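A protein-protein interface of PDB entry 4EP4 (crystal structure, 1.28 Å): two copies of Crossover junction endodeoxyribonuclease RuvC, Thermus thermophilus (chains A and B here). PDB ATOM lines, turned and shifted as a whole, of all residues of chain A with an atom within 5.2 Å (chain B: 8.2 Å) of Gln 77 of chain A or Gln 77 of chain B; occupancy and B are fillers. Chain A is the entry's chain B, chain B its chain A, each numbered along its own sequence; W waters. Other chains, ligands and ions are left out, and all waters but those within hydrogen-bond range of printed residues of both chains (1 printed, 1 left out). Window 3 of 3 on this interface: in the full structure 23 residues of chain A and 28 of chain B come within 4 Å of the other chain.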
ATOM      1  N   GLN A  72       1.437 -28.291  27.788  1.00  0.00           N
ATOM      2  CA  GLN A  72       2.269 -29.243  27.059  1.00  0.00           C
ATOM      3  C   GLN A  72       1.721 -29.351  25.644  1.00  0.00           C
ATOM      4  O   GLN A  72       0.537 -29.633  25.452  1.00  0.00           O
ATOM      5  CB  GLN A  72       2.248 -30.614  27.748  1.00  0.00           C
ATOM      6  CG  GLN A  72       3.178 -31.657  27.129  1.00  0.00           C
ATOM      7  CD  GLN A  72       3.133 -32.985  27.865  1.00  0.00           C
ATOM      8  OE1 GLN A  72       3.532 -33.076  29.027  1.00  0.00           O
ATOM      9  NE2 GLN A  72       2.641 -34.020  27.197  1.00  0.00           N
ATOM     10  N   PHE A  73       2.572 -29.114  24.652  1.00  0.00           N
ATOM     11  CA  PHE A  73       2.135 -29.162  23.264  1.00  0.00           C
ATOM     12  C   PHE A  73       3.051 -30.030  22.397  1.00  0.00           C
ATOM     13  O   PHE A  73       3.366 -29.660  21.265  1.00  0.00           O
ATOM     14  CB  PHE A  73       2.035 -27.748  22.678  1.00  0.00           C
ATOM     15  CG  PHE A  73       1.293 -26.775  23.556  1.00  0.00           C
ATOM     16  CD1 PHE A  73       1.978 -25.758  24.214  1.00  0.00           C
ATOM     17  CD2 PHE A  73      -0.079 -26.888  23.737  1.00  0.00           C
ATOM     18  CE1 PHE A  73       1.310 -24.862  25.034  1.00  0.00           C
ATOM     19  CE2 PHE A  73      -0.762 -25.996  24.557  1.00  0.00           C
ATOM     20  CZ  PHE A  73      -0.060 -24.979  25.206  1.00  0.00           C
ATOM     21  N   PHE A  74       3.464 -31.182  22.924  1.00  0.00           N
ATOM     22  CA  PHE A  74       4.249 -32.145  22.149  1.00  0.00           C
ATOM     23  C   PHE A  74       3.360 -32.675  21.029  1.00  0.00           C
ATOM     24  O   PHE A  74       2.143 -32.482  21.065  1.00  0.00           O
ATOM     25  CB  PHE A  74       4.702 -33.331  23.014  1.00  0.00           C
ATOM     26  CG  PHE A  74       5.519 -32.952  24.225  1.00  0.00           C
ATOM     27  CD1 PHE A  74       6.119 -31.703  24.329  1.00  0.00           C
ATOM     28  CD2 PHE A  74       5.690 -33.860  25.261  1.00  0.00           C
ATOM     29  CE1 PHE A  74       6.868 -31.365  25.451  1.00  0.00           C
ATOM     30  CE2 PHE A  74       6.435 -33.533  26.386  1.00  0.00           C
ATOM     31  CZ  PHE A  74       7.027 -32.284  26.481  1.00  0.00           C
ATOM     32  N   TYR A  75       3.948 -33.369  20.060  1.00  0.00           N
ATOM     33  CA  TYR A  75       3.162 -33.925  18.958  1.00  0.00           C
ATOM     34  C   TYR A  75       2.038 -34.840  19.466  1.00  0.00           C
ATOM     35  O   TYR A  75       0.873 -34.685  19.087  1.00  0.00           O
ATOM     36  CB  TYR A  75       4.065 -34.678  17.974  1.00  0.00           C
ATOM     37  CG  TYR A  75       3.305 -35.221  16.790  1.00  0.00           C
ATOM     38  CD1 TYR A  75       3.060 -34.427  15.677  1.00  0.00           C
ATOM     39  CD2 TYR A  75       2.804 -36.519  16.798  1.00  0.00           C
ATOM     40  CE1 TYR A  75       2.357 -34.914  14.593  1.00  0.00           C
ATOM     41  CE2 TYR A  75       2.096 -37.016  15.724  1.00  0.00           C
ATOM     42  CZ  TYR A  75       1.876 -36.213  14.624  1.00  0.00           C
ATOM     43  OH  TYR A  75       1.163 -36.715  13.563  1.00  0.00           O
ATOM     44  N   ARG A  76       2.397 -35.781  20.335  1.00  0.00           N
ATOM     45  CA  ARG A  76       1.409 -36.638  20.980  1.00  0.00           C
ATOM     46  C   ARG A  76       0.758 -35.897  22.145  1.00  0.00           C
ATOM     47  O   ARG A  76       1.438 -35.341  23.010  1.00  0.00           O
ATOM     48  CB  ARG A  76       2.047 -37.947  21.454  1.00  0.00           C
ATOM     49  CG  ARG A  76       2.605 -38.799  20.311  1.00  0.00           C
ATOM     50  CD  ARG A  76       1.484 -39.338  19.434  1.00  0.00           C
ATOM     51  NE  ARG A  76       0.586 -40.197  20.204  1.00  0.00           N
ATOM     52  CZ  ARG A  76       0.703 -41.520  20.293  1.00  0.00           C
ATOM     53  NH1 ARG A  76       1.671 -42.146  19.639  1.00  0.00           N
ATOM     54  NH2 ARG A  76      -0.158 -42.220  21.024  1.00  0.00           N
ATOM     55  N   GLN A  77      -0.570 -35.881  22.156  1.00  0.00           N
ATOM     56  CA  GLN A  77      -1.319 -35.192  23.209  1.00  0.00           C
ATOM     57  C   GLN A  77      -2.460 -36.084  23.682  1.00  0.00           C
ATOM     58  O   GLN A  77      -3.098 -36.734  22.869  1.00  0.00           O
ATOM     59  CB  GLN A  77      -1.900 -33.888  22.658  1.00  0.00           C
ATOM     60  CG  GLN A  77      -0.843 -32.863  22.287  1.00  0.00           C
ATOM     61  CD  GLN A  77      -1.321 -31.814  21.292  1.00  0.00           C
ATOM     62  OE1 GLN A  77      -2.526 -31.632  21.062  1.00  0.00           O
ATOM     63  NE2 GLN A  77      -0.366 -31.105  20.700  1.00  0.00           N
ATOM     64  N   ASN A  78      -2.728 -36.115  24.985  1.00  0.00           N
ATOM     65  CA  ASN A  78      -3.812 -36.951  25.504  1.00  0.00           C
ATOM     66  C   ASN A  78      -5.196 -36.545  24.986  1.00  0.00           C
ATOM     67  O   ASN A  78      -6.075 -37.385  24.781  1.00  0.00           O
ATOM     68  CB  ASN A  78      -3.796 -36.990  27.035  1.00  0.00           C
ATOM     69  CG  ASN A  78      -2.606 -37.756  27.585  1.00  0.00           C
ATOM     70  OD1 ASN A  78      -2.038 -38.618  26.907  1.00  0.00           O
ATOM     71  ND2 ASN A  78      -2.224 -37.452  28.822  1.00  0.00           N
ATOM     72  N   GLU A  79      -5.388 -35.251  24.773  1.00  0.00           N
ATOM     73  CA  GLU A  79      -6.623 -34.757  24.177  1.00  0.00           C
ATOM     74  C   GLU A  79      -6.249 -33.636  23.211  1.00  0.00           C
ATOM     75  O   GLU A  79      -5.181 -33.032  23.362  1.00  0.00           O
ATOM     76  CB  GLU A  79      -7.597 -34.268  25.254  1.00  0.00           C
ATOM     77  CG  GLU A  79      -8.077 -35.370  26.194  1.00  0.00           C
ATOM     78  CD  GLU A  79      -9.150 -34.911  27.143  1.00  0.00           C
ATOM     79  OE1 GLU A  79      -8.838 -34.164  28.088  1.00  0.00           O
ATOM     80  OE2 GLU A  79     -10.318 -35.294  26.937  1.00  0.00           O
ATOM     81  N   LEU A  80      -7.098 -33.387  22.215  1.00  0.00           N
ATOM     82  CA  LEU A  80      -6.831 -32.354  21.212  1.00  0.00           C
ATOM     83  C   LEU A  80      -6.524 -31.003  21.861  1.00  0.00           C
ATOM     84  O   LEU A  80      -7.271 -30.555  22.726  1.00  0.00           O
ATOM     85  CB  LEU A  80      -8.032 -32.204  20.275  1.00  0.00           C
ATOM     86  CG  LEU A  80      -8.398 -33.387  19.376  1.00  0.00           C
ATOM     87  CD1 LEU A  80      -9.683 -33.099  18.606  1.00  0.00           C
ATOM     88  CD2 LEU A  80      -7.267 -33.705  18.411  1.00  0.00           C
ATOM     89  N   ALA A  81      -5.433 -30.357  21.444  1.00  0.00           N
ATOM     90  CA  ALA A  81      -5.068 -29.037  21.976  1.00  0.00           C
ATOM     91  C   ALA A  81      -6.232 -28.046  21.904  1.00  0.00           C
ATOM     92  O   ALA A  81      -6.448 -27.258  22.826  1.00  0.00           O
ATOM     93  CB  ALA A  81      -3.842 -28.473  21.256  1.00  0.00           C
ATOM     94  N   TYR A  82      -6.989 -28.106  20.815  1.00  0.00           N
ATOM     95  CA  TYR A  82      -8.144 -27.243  20.636  1.00  0.00           C
ATOM     96  C   TYR A  82      -9.159 -27.410  21.770  1.00  0.00           C
ATOM     97  O   TYR A  82      -9.613 -26.426  22.356  1.00  0.00           O
ATOM     98  CB  TYR A  82      -8.783 -27.529  19.277  1.00  0.00           C
ATOM     99  CG  TYR A  82      -9.973 -26.677  18.931  1.00  0.00           C
ATOM    100  CD1 TYR A  82      -9.909 -25.284  18.997  1.00  0.00           C
ATOM    101  CD2 TYR A  82     -11.153 -27.264  18.492  1.00  0.00           C
ATOM    102  CE1 TYR A  82     -11.000 -24.507  18.653  1.00  0.00           C
ATOM    103  CE2 TYR A  82     -12.240 -26.494  18.145  1.00  0.00           C
ATOM    104  CZ  TYR A  82     -12.159 -25.123  18.227  1.00  0.00           C
ATOM    105  OH  TYR A  82     -13.249 -24.370  17.874  1.00  0.00           O
ATOM    106  N   GLN B  72     -13.779 -26.023  13.762  1.00  0.00           N
ATOM    107  CA  GLN B  72     -12.378 -25.732  13.488  1.00  0.00           C
ATOM    108  C   GLN B  72     -11.570 -27.001  13.280  1.00  0.00           C
ATOM    109  O   GLN B  72     -11.577 -27.901  14.129  1.00  0.00           O
ATOM    110  CB  GLN B  72     -11.769 -24.930  14.642  1.00  0.00           C
ATOM    111  CG  GLN B  72     -12.461 -23.596  14.912  1.00  0.00           C
ATOM    112  CD  GLN B  72     -11.713 -22.414  14.332  1.00  0.00           C
ATOM    113  OE1 GLN B  72     -10.572 -22.542  13.889  1.00  0.00           O
ATOM    114  NE2 GLN B  72     -12.349 -21.247  14.345  1.00  0.00           N
ATOM    115  N   PHE B  73     -10.861 -27.059  12.156  1.00  0.00           N
ATOM    116  CA  PHE B  73      -9.946 -28.157  11.887  1.00  0.00           C
ATOM    117  C   PHE B  73      -8.520 -27.634  11.873  1.00  0.00           C
ATOM    118  O   PHE B  73      -8.256 -26.523  11.396  1.00  0.00           O
ATOM    119  CB  PHE B  73     -10.270 -28.820  10.549  1.00  0.00           C
ATOM    120  CG  PHE B  73     -11.695 -29.278  10.428  1.00  0.00           C
ATOM    121  CD1 PHE B  73     -12.178 -30.312  11.221  1.00  0.00           C
ATOM    122  CD2 PHE B  73     -12.555 -28.676   9.517  1.00  0.00           C
ATOM    123  CE1 PHE B  73     -13.492 -30.736  11.111  1.00  0.00           C
ATOM    124  CE2 PHE B  73     -13.867 -29.090   9.401  1.00  0.00           C
ATOM    125  CZ  PHE B  73     -14.337 -30.123  10.199  1.00  0.00           C
ATOM    126  N   PHE B  74      -7.608 -28.429  12.414  1.00  0.00           N
ATOM    127  CA  PHE B  74      -6.201 -28.064  12.440  1.00  0.00           C
ATOM    128  C   PHE B  74      -5.378 -29.221  11.899  1.00  0.00           C
ATOM    129  O   PHE B  74      -5.523 -30.361  12.353  1.00  0.00           O
ATOM    130  CB  PHE B  74      -5.767 -27.724  13.867  1.00  0.00           C
ATOM    131  CG  PHE B  74      -6.526 -26.574  14.468  1.00  0.00           C
ATOM    132  CD1 PHE B  74      -6.112 -25.263  14.256  1.00  0.00           C
ATOM    133  CD2 PHE B  74      -7.668 -26.804  15.225  1.00  0.00           C
ATOM    134  CE1 PHE B  74      -6.817 -24.195  14.797  1.00  0.00           C
ATOM    135  CE2 PHE B  74      -8.386 -25.748  15.772  1.00  0.00           C
ATOM    136  CZ  PHE B  74      -7.961 -24.436  15.558  1.00  0.00           C
ATOM    137  N   TYR B  75      -4.528 -28.934  10.918  1.00  0.00           N
ATOM    138  CA  TYR B  75      -3.580 -29.925  10.437  1.00  0.00           C
ATOM    139  C   TYR B  75      -2.647 -30.329  11.571  1.00  0.00           C
ATOM    140  O   TYR B  75      -2.235 -31.488  11.665  1.00  0.00           O
ATOM    141  CB  TYR B  75      -2.763 -29.364   9.288  1.00  0.00           C
ATOM    142  CG  TYR B  75      -3.551 -29.126   8.024  1.00  0.00           C
ATOM    143  CD1 TYR B  75      -4.627 -29.936   7.684  1.00  0.00           C
ATOM    144  CD2 TYR B  75      -3.203 -28.103   7.156  1.00  0.00           C
ATOM    145  CE1 TYR B  75      -5.344 -29.718   6.520  1.00  0.00           C
ATOM    146  CE2 TYR B  75      -3.912 -27.878   5.991  1.00  0.00           C
ATOM    147  CZ  TYR B  75      -4.985 -28.687   5.680  1.00  0.00           C
ATOM    148  OH  TYR B  75      -5.697 -28.471   4.520  1.00  0.00           O
ATOM    149  N   ARG B  76      -2.308 -29.359  12.417  1.00  0.00           N
ATOM    150  CA  ARG B  76      -1.459 -29.588  13.581  1.00  0.00           C
ATOM    151  C   ARG B  76      -2.101 -29.018  14.839  1.00  0.00           C
ATOM    152  O   ARG B  76      -2.437 -27.830  14.895  1.00  0.00           O
ATOM    153  CB  ARG B  76      -0.079 -28.955  13.379  1.00  0.00           C
ATOM    154  CG  ARG B  76       0.886 -29.150  14.559  1.00  0.00           C
ATOM    155  CD  ARG B  76       1.355 -30.608  14.673  1.00  0.00           C
ATOM    156  NE  ARG B  76       1.958 -31.054  13.416  1.00  0.00           N
ATOM    157  CZ  ARG B  76       3.191 -30.753  13.025  1.00  0.00           C
ATOM    158  NH1 ARG B  76       3.634 -31.183  11.853  1.00  0.00           N
ATOM    159  NH2 ARG B  76       3.984 -30.025  13.804  1.00  0.00           N
ATOM    160  N   GLN B  77      -2.279 -29.875  15.839  1.00  0.00           N
ATOM    161  CA  GLN B  77      -2.750 -29.430  17.142  1.00  0.00           C
ATOM    162  C   GLN B  77      -1.542 -28.937  17.924  1.00  0.00           C
ATOM    163  O   GLN B  77      -0.608 -29.690  18.175  1.00  0.00           O
ATOM    164  CB  GLN B  77      -3.449 -30.563  17.890  1.00  0.00           C
ATOM    165  CG  GLN B  77      -4.751 -31.041  17.236  1.00  0.00           C
ATOM    166  CD  GLN B  77      -5.930 -30.100  17.473  1.00  0.00           C
ATOM    167  OE1 GLN B  77      -5.880 -29.216  18.339  1.00  0.00           O
ATOM    168  NE2 GLN B  77      -7.006 -30.294  16.712  1.00  0.00           N
ATOM    169  N   ASN B  78      -1.541 -27.655  18.264  1.00  0.00           N
ATOM    170  CA  ASN B  78      -0.461 -27.073  19.047  1.00  0.00           C
ATOM    171  C   ASN B  78      -0.967 -25.845  19.786  1.00  0.00           C
ATOM    172  O   ASN B  78      -2.177 -25.655  19.917  1.00  0.00           O
ATOM    173  CB  ASN B  78       0.739 -26.733  18.161  1.00  0.00           C
ATOM    174  CG  ASN B  78       0.382 -25.782  17.027  1.00  0.00           C
ATOM    175  OD1 ASN B  78      -0.637 -25.089  17.071  1.00  0.00           O
ATOM    176  ND2 ASN B  78       1.230 -25.742  16.002  1.00  0.00           N
ATOM    177  N   GLU B  79      -0.044 -25.016  20.266  1.00  0.00           N
ATOM    178  CA  GLU B  79      -0.416 -23.840  21.053  1.00  0.00           C
ATOM    179  C   GLU B  79      -1.369 -22.892  20.316  1.00  0.00           C
ATOM    180  O   GLU B  79      -2.210 -22.254  20.942  1.00  0.00           O
ATOM    181  CB  GLU B  79       0.826 -23.085  21.537  1.00  0.00           C
ATOM    182  CG  GLU B  79       0.520 -22.041  22.612  1.00  0.00           C
ATOM    183  CD  GLU B  79       1.765 -21.357  23.135  1.00  0.00           C
ATOM    184  OE1 GLU B  79       1.659 -20.632  24.149  1.00  0.00           O
ATOM    185  OE2 GLU B  79       2.843 -21.545  22.531  1.00  0.00           O
ATOM    186  N   LEU B  80      -1.250 -22.819  18.992  1.00  0.00           N
ATOM    187  CA  LEU B  80      -2.154 -21.991  18.191  1.00  0.00           C
ATOM    188  C   LEU B  80      -3.609 -22.443  18.325  1.00  0.00           C
ATOM    189  O   LEU B  80      -4.493 -21.639  18.631  1.00  0.00           O
ATOM    190  CB  LEU B  80      -1.731 -21.982  16.718  1.00  0.00           C
ATOM    191  CG  LEU B  80      -0.796 -20.863  16.261  1.00  0.00           C
ATOM    192  CD1 LEU B  80       0.371 -20.665  17.214  1.00  0.00           C
ATOM    193  CD2 LEU B  80      -0.307 -21.129  14.848  1.00  0.00           C
ATOM    194  N   ALA B  81      -3.845 -23.737  18.113  1.00  0.00           N
ATOM    195  CA  ALA B  81      -5.180 -24.309  18.225  1.00  0.00           C
ATOM    196  C   ALA B  81      -5.702 -24.144  19.650  1.00  0.00           C
ATOM    197  O   ALA B  81      -6.877 -23.845  19.862  1.00  0.00           O
ATOM    198  CB  ALA B  81      -5.161 -25.775  17.838  1.00  0.00           C
ATOM    199  N   TYR B  82      -4.814 -24.360  20.617  1.00  0.00           N
ATOM    200  CA  TYR B  82      -5.093 -24.186  22.039  1.00  0.00           C
ATOM    201  C   TYR B  82      -5.656 -22.793  22.323  1.00  0.00           C
ATOM    202  O   TYR B  82      -6.702 -22.650  22.961  1.00  0.00           O
ATOM    203  CB  TYR B  82      -3.778 -24.426  22.769  1.00  0.00           C
ATOM    204  CG  TYR B  82      -3.691 -24.176  24.258  1.00  0.00           C
ATOM    205  CD1 TYR B  82      -2.823 -23.204  24.753  1.00  0.00           C
ATOM    206  CD2 TYR B  82      -4.385 -24.960  25.173  1.00  0.00           C
ATOM    207  CE1 TYR B  82      -2.675 -22.992  26.109  1.00  0.00           C
ATOM    208  CE2 TYR B  82      -4.242 -24.754  26.541  1.00  0.00           C
ATOM    209  CZ  TYR B  82      -3.385 -23.768  26.997  1.00  0.00           C
ATOM    210  OH  TYR B  82      -3.218 -23.544  28.340  1.00  0.00           O
ATOM    211  N   GLY B  85      -9.004 -22.208  20.973  1.00  0.00           N
ATOM    212  CA  GLY B  85      -9.853 -22.917  21.909  1.00  0.00           C
ATOM    213  C   GLY B  85     -10.253 -22.083  23.114  1.00  0.00           C
ATOM    214  O   GLY B  85     -11.391 -22.174  23.562  1.00  0.00           O
HETATM  215  O   HOH W   1     -15.174 -25.639  16.474  1.00  0.00           O
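The backbone NH of Ala 81 of chain A lies within hydrogen-bond range of the side-chain amide oxygen of Gln 77 of chain B.
The side-chain amide oxygen (OE1) of Gln 77 of chain B sits at hydrogen-bond distance from the backbone NH (N) of Tyr 82 of chain A.
O of Gln 77 of chain B sits at hydrogen-bond distance from NE2 of Gln 77 of chain A (2.9 Å).
The backbone carbonyl oxygen (O) of Phe 74 of chain A lies within hydrogen-bond range of the side-chain amide nitrogen (NE2) of Gln 77 of chain A (2.9 Å).
The backbone NH (N) of Ala 81 of chain A is in hydrogen-bond range of the side-chain amide oxygen (OE1) of Gln 77 of chain A, at 3.2 Å.
The side-chain amide oxygen of Asn 78 of chain B sits at hydrogen-bond distance from the backbone NH of Leu 80 of chain B (3.0 Å).
Among the printed residues, merely in contact across the chains: Tyr 82 of chain A with Gln 72 of chain B, Phe 73 of chain A with Tyr 82 of chain B, Ala 81 of chain A with Tyr 82 of chain B, Tyr 82 of chain A with Ala 81 of chain B, Ala 81 of chain A with Asn 78 of chain B, Tyr 82 of chain A with Gly 85 of chain B, Tyr 82 of chain A with Phe 74 of chain B, Phe 73 of chain A with Glu 79 of chain B and Leu 80 of chain A with Gln 77 of chain B.
Of chain B, only Gln 77 comes within 4 Å of Gln 77 of chain A.
Of chain A, only Gln 77, Leu 80, Ala 81 and Tyr 82 come within 4 Å of Gln 77 of chain B.
Of the printed residues of chain A, Gln 72 of chain B touches Tyr 82.
Of the printed residues of chain B, Ala 81 of chain A touches Gln 77, Asn 78 and Tyr 82.
Of the printed residues of chain A, Phe 74 of chain B touches Tyr 82 (3.6 Å).
Of the printed residues of chain A, Tyr 82 of chain B touches Phe 73 (3.3 Å) and Ala 81 (3.4 Å).
The nearest printed residue of chain A that does not touch Gln 72 of chain B is Leu 80 of chain A (7.1 Å).
Hydrophobic or aromatic side chains of chain A that line the printed part of chain B: Phe 73, Leu 80, Ala 81 and Tyr 82.
Phe 73 of chain A touches Glu 79 of chain B, but with the chains exchanged Glu 79 of chain A does not touch Phe 73 of chain B (13.0 Å).
Phe 73 of chain A touches Tyr 82 of chain B, but with the chains exchanged Tyr 82 of chain A does not touch Phe 73 of chain B (6.2 Å).
Ala 81 of chain A touches Gln 77 of chain B, but with the chains exchanged Gln 77 of chain A does not touch Ala 81 of chain B (7.2 Å).
Tyr 82 of chain A touches Phe 74 of chain B, but with the chains exchanged Phe 74 of chain A does not touch Tyr 82 of chain B (9.9 Å).
11 positions are printed for both chains.
Of the 12 pairs that touch across the chains among the printed residues, 3 have their exchanged pair printed and touching as well.
Water W1 lies within hydrogen-bond range of the side-chain hydroxyl of Tyr 82 of chain A (2.7 Å) and the backbone NH of Gln 72 of chain B (3.1 Å).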
